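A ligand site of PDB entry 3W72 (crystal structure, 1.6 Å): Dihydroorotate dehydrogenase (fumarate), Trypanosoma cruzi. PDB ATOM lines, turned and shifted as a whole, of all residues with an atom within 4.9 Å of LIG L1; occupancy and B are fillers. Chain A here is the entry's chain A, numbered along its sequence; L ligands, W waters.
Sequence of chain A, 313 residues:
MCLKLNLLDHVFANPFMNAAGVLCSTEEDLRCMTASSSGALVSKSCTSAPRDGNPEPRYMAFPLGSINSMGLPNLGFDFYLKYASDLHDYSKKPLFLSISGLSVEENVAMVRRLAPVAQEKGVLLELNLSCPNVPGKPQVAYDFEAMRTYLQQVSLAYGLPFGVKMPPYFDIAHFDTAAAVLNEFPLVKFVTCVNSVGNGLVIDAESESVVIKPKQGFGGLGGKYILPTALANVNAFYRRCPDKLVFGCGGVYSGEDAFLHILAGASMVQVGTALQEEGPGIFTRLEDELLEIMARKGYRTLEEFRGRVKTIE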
ATOM      1  N   ALA A  19      17.254   9.024 -30.589  1.00  0.00           N
ATOM      2  CA  ALA A  19      18.034   8.530 -29.495  1.00  0.00           C
ATOM      3  C   ALA A  19      18.356   9.658 -28.556  1.00  0.00           C
ATOM      4  O   ALA A  19      18.665  10.771 -29.003  1.00  0.00           O
ATOM      5  CB  ALA A  19      19.291   7.868 -30.004  1.00  0.00           C
ATOM      6  N   ALA A  20      18.357   9.409 -27.228  1.00  0.00           N
ATOM      7  CA  ALA A  20      18.736  10.437 -26.333  1.00  0.00           C
ATOM      8  C   ALA A  20      20.083  11.033 -26.659  1.00  0.00           C
ATOM      9  O   ALA A  20      21.027  10.307 -27.043  1.00  0.00           O
ATOM     10  CB  ALA A  20      18.687   9.941 -24.885  1.00  0.00           C
ATOM     11  N   GLY A  21      20.214  12.307 -26.524  1.00  0.00           N
ATOM     12  CA  GLY A  21      21.418  12.989 -26.890  1.00  0.00           C
ATOM     13  C   GLY A  21      21.513  13.593 -28.244  1.00  0.00           C
ATOM     14  O   GLY A  21      22.240  14.552 -28.446  1.00  0.00           O
ATOM     15  N   VAL A  22      20.704  13.087 -29.179  1.00  0.00           N
ATOM     16  CA  VAL A  22      20.697  13.600 -30.581  1.00  0.00           C
ATOM     17  C   VAL A  22      19.457  14.434 -30.823  1.00  0.00           C
ATOM     18  O   VAL A  22      18.314  14.000 -30.588  1.00  0.00           O
ATOM     19  CB  VAL A  22      20.792  12.439 -31.587  1.00  0.00           C
ATOM     20  CG1 VAL A  22      20.720  13.004 -33.008  1.00  0.00           C
ATOM     21  CG2 VAL A  22      22.006  11.625 -31.330  1.00  0.00           C
ATOM     22  N   LYS A  44      17.502  15.221 -24.003  1.00  0.00           N
ATOM     23  CA  LYS A  44      18.885  14.922 -23.647  1.00  0.00           C
ATOM     24  C   LYS A  44      18.945  14.499 -22.164  1.00  0.00           C
ATOM     25  O   LYS A  44      18.350  15.169 -21.287  1.00  0.00           O
ATOM     26  CB  LYS A  44      19.672  16.245 -23.801  1.00  0.00           C
ATOM     27  CG  LYS A  44      21.075  16.259 -23.284  1.00  0.00           C
ATOM     28  CD  LYS A  44      22.070  15.300 -23.996  1.00  0.00           C
ATOM     29  CE  LYS A  44      23.454  15.088 -23.375  1.00  0.00           C
ATOM     30  NZ  LYS A  44      24.296  14.011 -24.080  1.00  0.00           N
ATOM     31  N   SER A  45      19.778  13.510 -21.897  1.00  0.00           N
ATOM     32  CA  SER A  45      19.962  13.045 -20.477  1.00  0.00           C
ATOM     33  C   SER A  45      20.457  14.272 -19.705  1.00  0.00           C
ATOM     34  O   SER A  45      21.397  14.935 -20.079  1.00  0.00           O
ATOM     35  CB  SER A  45      21.001  11.967 -20.337  1.00  0.00           C
ATOM     36  OG  SER A  45      20.486  10.784 -20.966  1.00  0.00           O
ATOM     37  N   TYR A  59      32.409  15.105 -30.876  1.00  0.00           N
ATOM     38  CA  TYR A  59      31.653  14.217 -31.742  1.00  0.00           C
ATOM     39  C   TYR A  59      32.254  14.270 -33.105  1.00  0.00           C
ATOM     40  O   TYR A  59      32.511  15.303 -33.630  1.00  0.00           O
ATOM     41  CB  TYR A  59      30.191  14.609 -31.821  1.00  0.00           C
ATOM     42  CG  TYR A  59      29.376  13.907 -32.892  1.00  0.00           C
ATOM     43  CD1 TYR A  59      28.766  12.689 -32.605  1.00  0.00           C
ATOM     44  CD2 TYR A  59      29.209  14.382 -34.176  1.00  0.00           C
ATOM     45  CE1 TYR A  59      28.025  12.047 -33.520  1.00  0.00           C
ATOM     46  CE2 TYR A  59      28.464  13.711 -35.098  1.00  0.00           C
ATOM     47  CZ  TYR A  59      27.929  12.534 -34.804  1.00  0.00           C
ATOM     48  OH  TYR A  59      27.153  11.842 -35.709  1.00  0.00           O
ATOM     49  N   SER A  66      29.865   6.769 -35.746  1.00  0.00           N
ATOM     50  CA  SER A  66      30.266   7.972 -35.007  1.00  0.00           C
ATOM     51  C   SER A  66      30.951   7.630 -33.704  1.00  0.00           C
ATOM     52  O   SER A  66      30.875   6.505 -33.182  1.00  0.00           O
ATOM     53  CB  SER A  66      29.022   8.827 -34.681  1.00  0.00           C
ATOM     54  OG  SER A  66      28.267   8.207 -33.655  1.00  0.00           O
ATOM     55  N   ASN A  68      31.775   9.636 -29.836  1.00  0.00           N
ATOM     56  CA  ASN A  68      31.516  10.848 -29.021  1.00  0.00           C
ATOM     57  C   ASN A  68      31.958  10.646 -27.620  1.00  0.00           C
ATOM     58  O   ASN A  68      31.867   9.607 -26.967  1.00  0.00           O
ATOM     59  CB  ASN A  68      30.045  11.230 -29.050  1.00  0.00           C
ATOM     60  CG  ASN A  68      29.239  10.584 -27.978  1.00  0.00           C
ATOM     61  OD1 ASN A  68      29.177  10.938 -26.782  1.00  0.00           O
ATOM     62  ND2 ASN A  68      28.602   9.487 -28.371  1.00  0.00           N
ATOM     63  N   MET A  70      30.844  13.519 -25.284  1.00  0.00           N
ATOM     64  CA  MET A  70      30.247  14.834 -25.094  1.00  0.00           C
ATOM     65  C   MET A  70      30.444  15.385 -23.758  1.00  0.00           C
ATOM     66  O   MET A  70      30.526  16.604 -23.675  1.00  0.00           O
ATOM     67  CB  MET A  70      28.784  14.759 -25.440  1.00  0.00           C
ATOM     68  CG  MET A  70      28.378  14.220 -26.769  1.00  0.00           C
ATOM     69  SD  MET A  70      29.016  15.124 -28.181  1.00  0.00           S
ATOM     70  CE  MET A  70      28.077  16.532 -28.189  1.00  0.00           C
ATOM     71  N   LEU A  72      28.180  14.975 -21.345  1.00  0.00           N
ATOM     72  CA  LEU A  72      26.834  15.295 -20.919  1.00  0.00           C
ATOM     73  C   LEU A  72      26.553  16.813 -20.886  1.00  0.00           C
ATOM     74  O   LEU A  72      26.037  17.321 -19.872  1.00  0.00           O
ATOM     75  CB  LEU A  72      26.435  14.600 -19.600  1.00  0.00           C
ATOM     76  CG  LEU A  72      24.934  14.545 -19.499  1.00  0.00           C
ATOM     77  CD1 LEU A  72      24.351  13.288 -20.134  1.00  0.00           C
ATOM     78  CD2 LEU A  72      24.496  14.552 -18.024  1.00  0.00           C
ATOM     79  N   SER A  98      14.925  11.999 -20.340  1.00  0.00           N
ATOM     80  CA  SER A  98      16.027  11.200 -19.903  1.00  0.00           C
ATOM     81  C   SER A  98      16.772  11.877 -18.775  1.00  0.00           C
ATOM     82  O   SER A  98      17.057  13.077 -18.854  1.00  0.00           O
ATOM     83  CB  SER A  98      16.977  10.843 -21.036  1.00  0.00           C
ATOM     84  OG  SER A  98      18.052  10.060 -20.564  1.00  0.00           O
ATOM     85  N   GLU A 126      12.993   7.988 -18.922  1.00  0.00           N
ATOM     86  CA  GLU A 126      14.056   7.065 -19.311  1.00  0.00           C
ATOM     87  C   GLU A 126      15.270   7.345 -18.454  1.00  0.00           C
ATOM     88  O   GLU A 126      15.799   8.365 -18.496  1.00  0.00           O
ATOM     89  CB  GLU A 126      14.421   7.150 -20.836  1.00  0.00           C
ATOM     90  CG  GLU A 126      15.336   6.048 -21.415  1.00  0.00           C
ATOM     91  CD  GLU A 126      15.673   6.159 -22.954  1.00  0.00           C
ATOM     92  OE1 GLU A 126      16.488   6.986 -23.351  1.00  0.00           O
ATOM     93  OE2 GLU A 126      15.125   5.392 -23.727  1.00  0.00           O
ATOM     94  N   ASN A 128      18.988   6.847 -17.615  1.00  0.00           N
ATOM     95  CA  ASN A 128      20.226   6.458 -18.279  1.00  0.00           C
ATOM     96  C   ASN A 128      21.174   5.873 -17.280  1.00  0.00           C
ATOM     97  O   ASN A 128      21.759   6.619 -16.523  1.00  0.00           O
ATOM     98  CB  ASN A 128      20.805   7.662 -19.008  1.00  0.00           C
ATOM     99  CG  ASN A 128      22.141   7.436 -19.669  1.00  0.00           C
ATOM    100  OD1 ASN A 128      22.661   6.343 -19.654  1.00  0.00           O
ATOM    101  ND2 ASN A 128      22.675   8.463 -20.314  1.00  0.00           N
ATOM    102  N   LYS A 165      17.780   3.039 -19.916  1.00  0.00           N
ATOM    103  CA  LYS A 165      18.639   2.960 -21.047  1.00  0.00           C
ATOM    104  C   LYS A 165      19.900   2.235 -20.607  1.00  0.00           C
ATOM    105  O   LYS A 165      20.589   2.646 -19.650  1.00  0.00           O
ATOM    106  CB  LYS A 165      18.978   4.339 -21.456  1.00  0.00           C
ATOM    107  CG  LYS A 165      20.034   4.515 -22.586  1.00  0.00           C
ATOM    108  CD  LYS A 165      19.440   4.206 -23.922  1.00  0.00           C
ATOM    109  CE  LYS A 165      20.313   4.568 -25.099  1.00  0.00           C
ATOM    110  NZ  LYS A 165      20.331   5.997 -25.379  1.00  0.00           N
ATOM    111  N   VAL A 194      20.552  -0.139 -27.351  1.00  0.00           N
ATOM    112  CA  VAL A 194      21.668   0.060 -26.490  1.00  0.00           C
ATOM    113  C   VAL A 194      22.160   1.516 -26.578  1.00  0.00           C
ATOM    114  O   VAL A 194      21.931   2.231 -27.563  1.00  0.00           O
ATOM    115  CB  VAL A 194      22.856  -0.855 -26.798  1.00  0.00           C
ATOM    116  CG1 VAL A 194      22.481  -2.322 -26.530  1.00  0.00           C
ATOM    117  CG2 VAL A 194      23.347  -0.675 -28.212  1.00  0.00           C
ATOM    118  N   ASN A 195      22.845   1.934 -25.506  1.00  0.00           N
ATOM    119  CA  ASN A 195      23.771   3.095 -25.556  1.00  0.00           C
ATOM    120  C   ASN A 195      24.987   2.774 -26.429  1.00  0.00           C
ATOM    121  O   ASN A 195      25.099   1.670 -26.952  1.00  0.00           O
ATOM    122  CB  ASN A 195      24.103   3.448 -24.092  1.00  0.00           C
ATOM    123  CG  ASN A 195      24.300   4.938 -23.900  1.00  0.00           C
ATOM    124  OD1 ASN A 195      24.940   5.619 -24.715  1.00  0.00           O
ATOM    125  ND2 ASN A 195      23.764   5.428 -22.839  1.00  0.00           N
ATOM    126  N   SER A 196      25.818   3.760 -26.618  1.00  0.00           N
ATOM    127  CA  SER A 196      26.959   3.557 -27.423  1.00  0.00           C
ATOM    128  C   SER A 196      27.860   2.449 -26.928  1.00  0.00           C
ATOM    129  O   SER A 196      27.894   2.115 -25.794  1.00  0.00           O
ATOM    130  CB  SER A 196      27.694   4.893 -27.656  1.00  0.00           C
ATOM    131  OG  SER A 196      27.935   5.551 -26.502  1.00  0.00           O
ATOM    132  N   GLY A 222      28.707   4.741 -32.216  1.00  0.00           N
ATOM    133  CA  GLY A 222      27.389   4.464 -32.702  1.00  0.00           C
ATOM    134  C   GLY A 222      27.442   4.248 -34.194  1.00  0.00           C
ATOM    135  O   GLY A 222      28.486   4.390 -34.830  1.00  0.00           O
ATOM    136  N   GLY A 223      26.248   3.938 -34.740  1.00  0.00           N
ATOM    137  CA  GLY A 223      26.116   3.740 -36.123  1.00  0.00           C
ATOM    138  C   GLY A 223      26.337   2.321 -36.625  1.00  0.00           C
ATOM    139  O   GLY A 223      26.035   1.385 -35.955  1.00  0.00           O
ATOM    140  N   ILE A 226      27.760  -0.765 -34.805  1.00  0.00           N
ATOM    141  CA  ILE A 226      27.159  -1.328 -33.606  1.00  0.00           C
ATOM    142  C   ILE A 226      25.840  -2.095 -33.830  1.00  0.00           C
ATOM    143  O   ILE A 226      25.273  -2.602 -32.906  1.00  0.00           O
ATOM    144  CB  ILE A 226      26.981  -0.341 -32.463  1.00  0.00           C
ATOM    145  CG1 ILE A 226      25.790   0.535 -32.593  1.00  0.00           C
ATOM    146  CG2 ILE A 226      28.270   0.438 -32.276  1.00  0.00           C
ATOM    147  CD1 ILE A 226      25.415   1.229 -31.327  1.00  0.00           C
ATOM    148  N   CYS A 249      17.905   0.594 -30.065  1.00  0.00           N
ATOM    149  CA  CYS A 249      18.677   1.684 -30.465  1.00  0.00           C
ATOM    150  C   CYS A 249      20.004   1.163 -30.853  1.00  0.00           C
ATOM    151  O   CYS A 249      20.583   0.360 -30.171  1.00  0.00           O
ATOM    152  CB  CYS A 249      18.889   2.620 -29.249  1.00  0.00           C
ATOM    153  SG  CYS A 249      19.660   4.182 -29.688  1.00  0.00           S
ATOM    154  N   GLY A 250      20.479   1.553 -31.995  1.00  0.00           N
ATOM    155  CA  GLY A 250      21.826   1.247 -32.438  1.00  0.00           C
ATOM    156  C   GLY A 250      21.885   0.874 -33.874  1.00  0.00           C
ATOM    157  O   GLY A 250      21.278  -0.130 -34.288  1.00  0.00           O
ATOM    158  N   GLY A 251      22.547   1.669 -34.705  1.00  0.00           N
ATOM    159  CA  GLY A 251      22.806   1.253 -36.052  1.00  0.00           C
ATOM    160  C   GLY A 251      21.662   1.387 -37.003  1.00  0.00           C
ATOM    161  O   GLY A 251      21.743   0.809 -38.126  1.00  0.00           O
ATOM    162  N   VAL A 252      20.608   2.134 -36.663  1.00  0.00           N
ATOM    163  CA  VAL A 252      19.475   2.258 -37.575  1.00  0.00           C
ATOM    164  C   VAL A 252      19.789   3.372 -38.596  1.00  0.00           C
ATOM    165  O   VAL A 252      19.829   4.543 -38.226  1.00  0.00           O
ATOM    166  CB  VAL A 252      18.185   2.514 -36.837  1.00  0.00           C
ATOM    167  CG1 VAL A 252      17.019   2.755 -37.846  1.00  0.00           C
ATOM    168  CG2 VAL A 252      17.869   1.325 -35.895  1.00  0.00           C
ATOM    169  N   GLN A 270      14.889   3.696 -31.972  1.00  0.00           N
ATOM    170  CA  GLN A 270      15.538   4.978 -31.723  1.00  0.00           C
ATOM    171  C   GLN A 270      16.651   5.164 -32.739  1.00  0.00           C
ATOM    172  O   GLN A 270      17.297   4.194 -33.120  1.00  0.00           O
ATOM    173  CB  GLN A 270      16.100   5.148 -30.345  1.00  0.00           C
ATOM    174  CG  GLN A 270      15.102   4.771 -29.220  1.00  0.00           C
ATOM    175  CD  GLN A 270      15.581   5.133 -27.880  1.00  0.00           C
ATOM    176  OE1 GLN A 270      16.804   5.274 -27.658  1.00  0.00           O
ATOM    177  NE2 GLN A 270      14.646   5.437 -26.985  1.00  0.00           N
ATOM    178  N   VAL A 271      16.865   6.405 -33.156  1.00  0.00           N
ATOM    179  CA  VAL A 271      17.787   6.717 -34.223  1.00  0.00           C
ATOM    180  C   VAL A 271      18.759   7.792 -33.718  1.00  0.00           C
ATOM    181  O   VAL A 271      18.337   8.880 -33.336  1.00  0.00           O
ATOM    182  CB  VAL A 271      17.052   7.216 -35.460  1.00  0.00           C
ATOM    183  CG1 VAL A 271      18.043   7.436 -36.568  1.00  0.00           C
ATOM    184  CG2 VAL A 271      15.958   6.189 -35.889  1.00  0.00           C
ATOM    185  N   GLY A 272      20.029   7.469 -33.569  1.00  0.00           N
ATOM    186  CA  GLY A 272      21.071   8.370 -33.105  1.00  0.00           C
ATOM    187  C   GLY A 272      21.952   8.937 -34.135  1.00  0.00           C
ATOM    188  O   GLY A 272      21.576   9.932 -34.768  1.00  0.00           O
ATOM    189  N   THR A 273      23.045   8.255 -34.420  1.00  0.00           N
ATOM    190  CA  THR A 273      23.975   8.721 -35.442  1.00  0.00           C
ATOM    191  C   THR A 273      23.330   9.045 -36.730  1.00  0.00           C
ATOM    192  O   THR A 273      23.656  10.097 -37.334  1.00  0.00           O
ATOM    193  CB  THR A 273      25.110   7.632 -35.633  1.00  0.00           C
ATOM    194  OG1 THR A 273      25.765   7.410 -34.395  1.00  0.00           O
ATOM    195  CG2 THR A 273      26.083   8.062 -36.747  1.00  0.00           C
ATOM    196  N   ALA A 274      22.471   8.187 -37.250  1.00  0.00           N
ATOM    197  CA  ALA A 274      21.943   8.512 -38.602  1.00  0.00           C
ATOM    198  C   ALA A 274      21.093   9.796 -38.609  1.00  0.00           C
ATOM    199  O   ALA A 274      21.021  10.472 -39.595  1.00  0.00           O
ATOM    200  CB  ALA A 274      21.104   7.351 -39.117  1.00  0.00           C
HETATM  201  N1  LIG L   1      22.490   8.299 -24.843  1.00  0.00           N
HETATM  202  C1  LIG L   1      21.840   8.631 -23.711  1.00  0.00           C
HETATM  203  O1  LIG L   1      21.054   7.835 -23.185  1.00  0.00           O
HETATM  204  N2  LIG L   1      21.893   9.892 -23.240  1.00  0.00           N
HETATM  205  C2  LIG L   1      22.551  10.830 -23.825  1.00  0.00           C
HETATM  206  O2  LIG L   1      22.587  12.022 -23.358  1.00  0.00           O
HETATM  207  C3  LIG L   1      23.336  10.555 -25.007  1.00  0.00           C
HETATM  208  N3  LIG L   1      24.081  11.480 -25.628  1.00  0.00           N
HETATM  209  C4  LIG L   1      24.504  11.224 -26.850  1.00  0.00           C
HETATM  210  C5  LIG L   1      25.135  12.171 -27.606  1.00  0.00           C
HETATM  211  C6  LIG L   1      25.612  11.967 -28.859  1.00  0.00           C
HETATM  212  C7  LIG L   1      26.296  13.049 -29.649  1.00  0.00           C
HETATM  213  C8  LIG L   1      25.513  10.673 -29.389  1.00  0.00           C
HETATM  214  C9  LIG L   1      25.989  10.301 -30.720  1.00  0.00           C
HETATM  215  C10 LIG L   1      24.916   9.671 -28.635  1.00  0.00           C
HETATM  216  C11 LIG L   1      24.420   9.886 -27.379  1.00  0.00           C
HETATM  217  N4  LIG L   1      23.803   8.893 -26.654  1.00  0.00           N
HETATM  218  C12 LIG L   1      23.210   9.177 -25.473  1.00  0.00           C
HETATM  219  C13 LIG L   1      23.696   7.508 -27.141  1.00  0.00           C
HETATM  220  C14 LIG L   1      22.614   7.411 -28.155  1.00  0.00           C
HETATM  221  O3  LIG L   1      21.337   7.639 -27.536  1.00  0.00           O
HETATM  222  C15 LIG L   1      22.551   6.017 -28.768  1.00  0.00           C
HETATM  223  O4  LIG L   1      22.322   5.042 -27.719  1.00  0.00           O
HETATM  224  C16 LIG L   1      23.836   5.612 -29.478  1.00  0.00           C
HETATM  225  O5  LIG L   1      24.339   6.691 -30.254  1.00  0.00           O
HETATM  226  C17 LIG L   1      23.563   4.356 -30.374  1.00  0.00           C
HETATM  227  O6  LIG L   1      22.663   4.648 -31.428  1.00  0.00           O
HETATM  228  P1  LIG L   1      23.092   4.949 -32.938  1.00  0.00           P
HETATM  229  O7  LIG L   1      21.849   5.191 -33.627  1.00  0.00           O
HETATM  230  O8  LIG L   1      23.873   3.783 -33.436  1.00  0.00           O
HETATM  231  O9  LIG L   1      23.989   6.161 -32.832  1.00  0.00           O
HETATM  232  O1  LG2 L   2      29.008  11.804 -23.536  1.00  0.00           O
HETATM  233  C1  LG2 L   2      27.797  11.879 -23.331  1.00  0.00           C
HETATM  234  O2  LG2 L   2      27.044  12.900 -23.223  1.00  0.00           O
HETATM  235  C2  LG2 L   2      27.074  10.577 -23.593  1.00  0.00           C
HETATM  236  N1  LG2 L   2      27.344   9.932 -24.837  1.00  0.00           N
HETATM  237  C3  LG2 L   2      26.795   8.665 -25.115  1.00  0.00           C
HETATM  238  O3  LG2 L   2      27.062   8.126 -26.233  1.00  0.00           O
HETATM  239  N2  LG2 L   2      25.958   8.111 -24.258  1.00  0.00           N
HETATM  240  C4  LG2 L   2      25.623   8.712 -23.012  1.00  0.00           C
HETATM  241  O4  LG2 L   2      24.842   8.065 -22.279  1.00  0.00           O
HETATM  242  C5  LG2 L   2      26.284   9.959 -22.658  1.00  0.00           C
HETATM  243  C6  LG2 L   2      26.082  10.533 -21.309  1.00  0.00           C
HETATM  244  C7  LG2 L   2      26.673   9.588 -20.218  1.00  0.00           C
HETATM  245  C8  LG2 L   2      26.829  10.344 -18.949  1.00  0.00           C
HETATM  246  C9  LG2 L   2      27.956  11.184 -18.673  1.00  0.00           C
HETATM  247  C10 LG2 L   2      28.995  11.289 -19.562  1.00  0.00           C
HETATM  248  C11 LG2 L   2      30.075  12.155 -19.291  1.00  0.00           C
HETATM  249  C12 LG2 L   2      30.064  12.878 -18.066  1.00  0.00           C
HETATM  250  C13 LG2 L   2      29.027  12.797 -17.192  1.00  0.00           C
HETATM  251  C14 LG2 L   2      27.972  11.874 -17.456  1.00  0.00           C
HETATM  252  C15 LG2 L   2      26.910  11.756 -16.590  1.00  0.00           C
HETATM  253  C16 LG2 L   2      25.863  10.870 -16.744  1.00  0.00           C
HETATM  254  C17 LG2 L   2      25.840  10.200 -17.957  1.00  0.00           C
HETATM  255  O   HOH W   1      19.835   3.458 -34.061  1.00  0.00           O
HETATM  256  O   HOH W   2      26.970   6.618 -29.749  1.00  0.00           O
HETATM  257  O   HOH W   3      21.801   5.669 -36.358  1.00  0.00           O
HETATM  258  O   HOH W   4      18.550   7.872 -21.846  1.00  0.00           O
HETATM  259  O   HOH W   5      24.478  15.380 -26.670  1.00  0.00           O
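N of Thr 273 is in hydrogen-bond range of O9 of LIG L1, at 2.8 Å. An oxygen (O9) of LIG L1 is in hydrogen-bond range of the side-chain hydroxyl (OG1) of Thr 273. The backbone NH (N) of Gly 223 sits at hydrogen-bond distance from an oxygen (O8) of LIG L1 (2.7 Å). O2 of LIG L1 is in hydrogen-bond range of NZ of Lys 44 (2.7 Å). The backbone NH of Ala 20 is in hydrogen-bond range of an oxygen (O3) of LIG L1. An oxygen (O3) of LIG L1 sits at hydrogen-bond distance from the backbone carbonyl oxygen of Ala 20 (2.7 Å). The backbone NH of Gly 251 sits at hydrogen-bond distance from an oxygen (O8) of LIG L1 (2.8 Å). O2 of LIG L1 lies close to N of Ser 45 (3.5 Å). OG of Ser 45 is in hydrogen-bond range of N2 of LIG L1. O of Val 194 sits at hydrogen-bond distance from O4 of LIG L1, 2.8 Å away. The side-chain amino group (NZ) of Lys 165 lies within hydrogen-bond range of an oxygen (O3) of LIG L1, 2.9 Å away. N of Gly 272 sits at hydrogen-bond distance from O7 of LIG L1 (2.9 Å). ND2 of Asn 128 lies close to N2 of LIG L1 (3.3 Å). An oxygen (O4) of LIG L1 is in hydrogen-bond range of the side-chain sulfur (SG) of Cys 249. NZ of Lys 44 is in salt-bridge range of O2 of LG2 L2, at 3.1 Å. OD1 of Asn 195 is in hydrogen-bond range of N2 of LG2 L2 (2.7 Å). The side-chain amide nitrogen of Asn 128 lies within hydrogen-bond range of an oxygen (O4) of LG2 L2 (3.0 Å). N1 of LG2 L2 sits at hydrogen-bond distance from OD1 of Asn 68 (2.9 Å). The backbone NH (N) of Met 70 is in hydrogen-bond range of an oxygen (O1) of LG2 L2 (3.1 Å). O3 of LG2 L2 sits at hydrogen-bond distance from OG of Ser 196 (2.7 Å). O2 of LG2 L2 is in hydrogen-bond range of N of Leu 72.
Residues that only touch LIG L1: Ala 19 (3.2 Å), Asn 195 (3.3 Å), Gly 21 (3.3 Å), Gly 250 (3.4 Å), Asn 68 (3.5 Å), Ile 226 (3.7 Å), Gly 222 (3.7 Å), Met 70 (3.7 Å), Tyr 59 (3.9 Å), Ser 196 (3.9 Å) and Leu 72 (3.9 Å). Of the 30 residues printed, 22 come within 4 Å of LIG L1. Along chain A the residues within 4 Å of LIG L1 span positions 19 to 273.
OG of Ser 66 is in hydrogen-bond range of OG1 of Thr 273, 2.7 Å away. ND2 of Asn 128 lies within hydrogen-bond range of OG of Ser 45, 3.3 Å away. O of Cys 249 is in hydrogen-bond range of N of Val 194. The side-chain amide oxygen (OD1) of Asn 128 is in hydrogen-bond range of the side-chain amide nitrogen (ND2) of Asn 195, at 3.5 Å. The side-chain hydroxyl (OG) of Ser 196 lies within hydrogen-bond range of the side-chain amide oxygen (OD1) of Asn 195 (3.5 Å). The side-chain sulfur (SG) of Cys 249 sits at hydrogen-bond distance from the side-chain amide oxygen (OE1) of Gln 270. N of Met 70 sits close to OD1 of Asn 68. The backbone carbonyl oxygen of Gly 222 is in hydrogen-bond range of the backbone NH of Ser 66 (2.9 Å).
Water W3 lies within hydrogen-bond range of N of Ala 274 (2.8 Å), O7 of LIG L1 (2.8 Å), O of Val 252 (2.9 Å) and N of Thr 273 (3.5 Å). Water W4 lies within hydrogen-bond range of the side-chain hydroxyl of Ser 98 (2.6 Å), the side-chain carboxylate of Glu 126 (2.7 Å) and an oxygen (O1) of LIG L1 (2.8 Å). Water W5 lies within hydrogen-bond range of NZ of Lys 44 (2.9 Å) and O of Gly 21 (3.0 Å).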
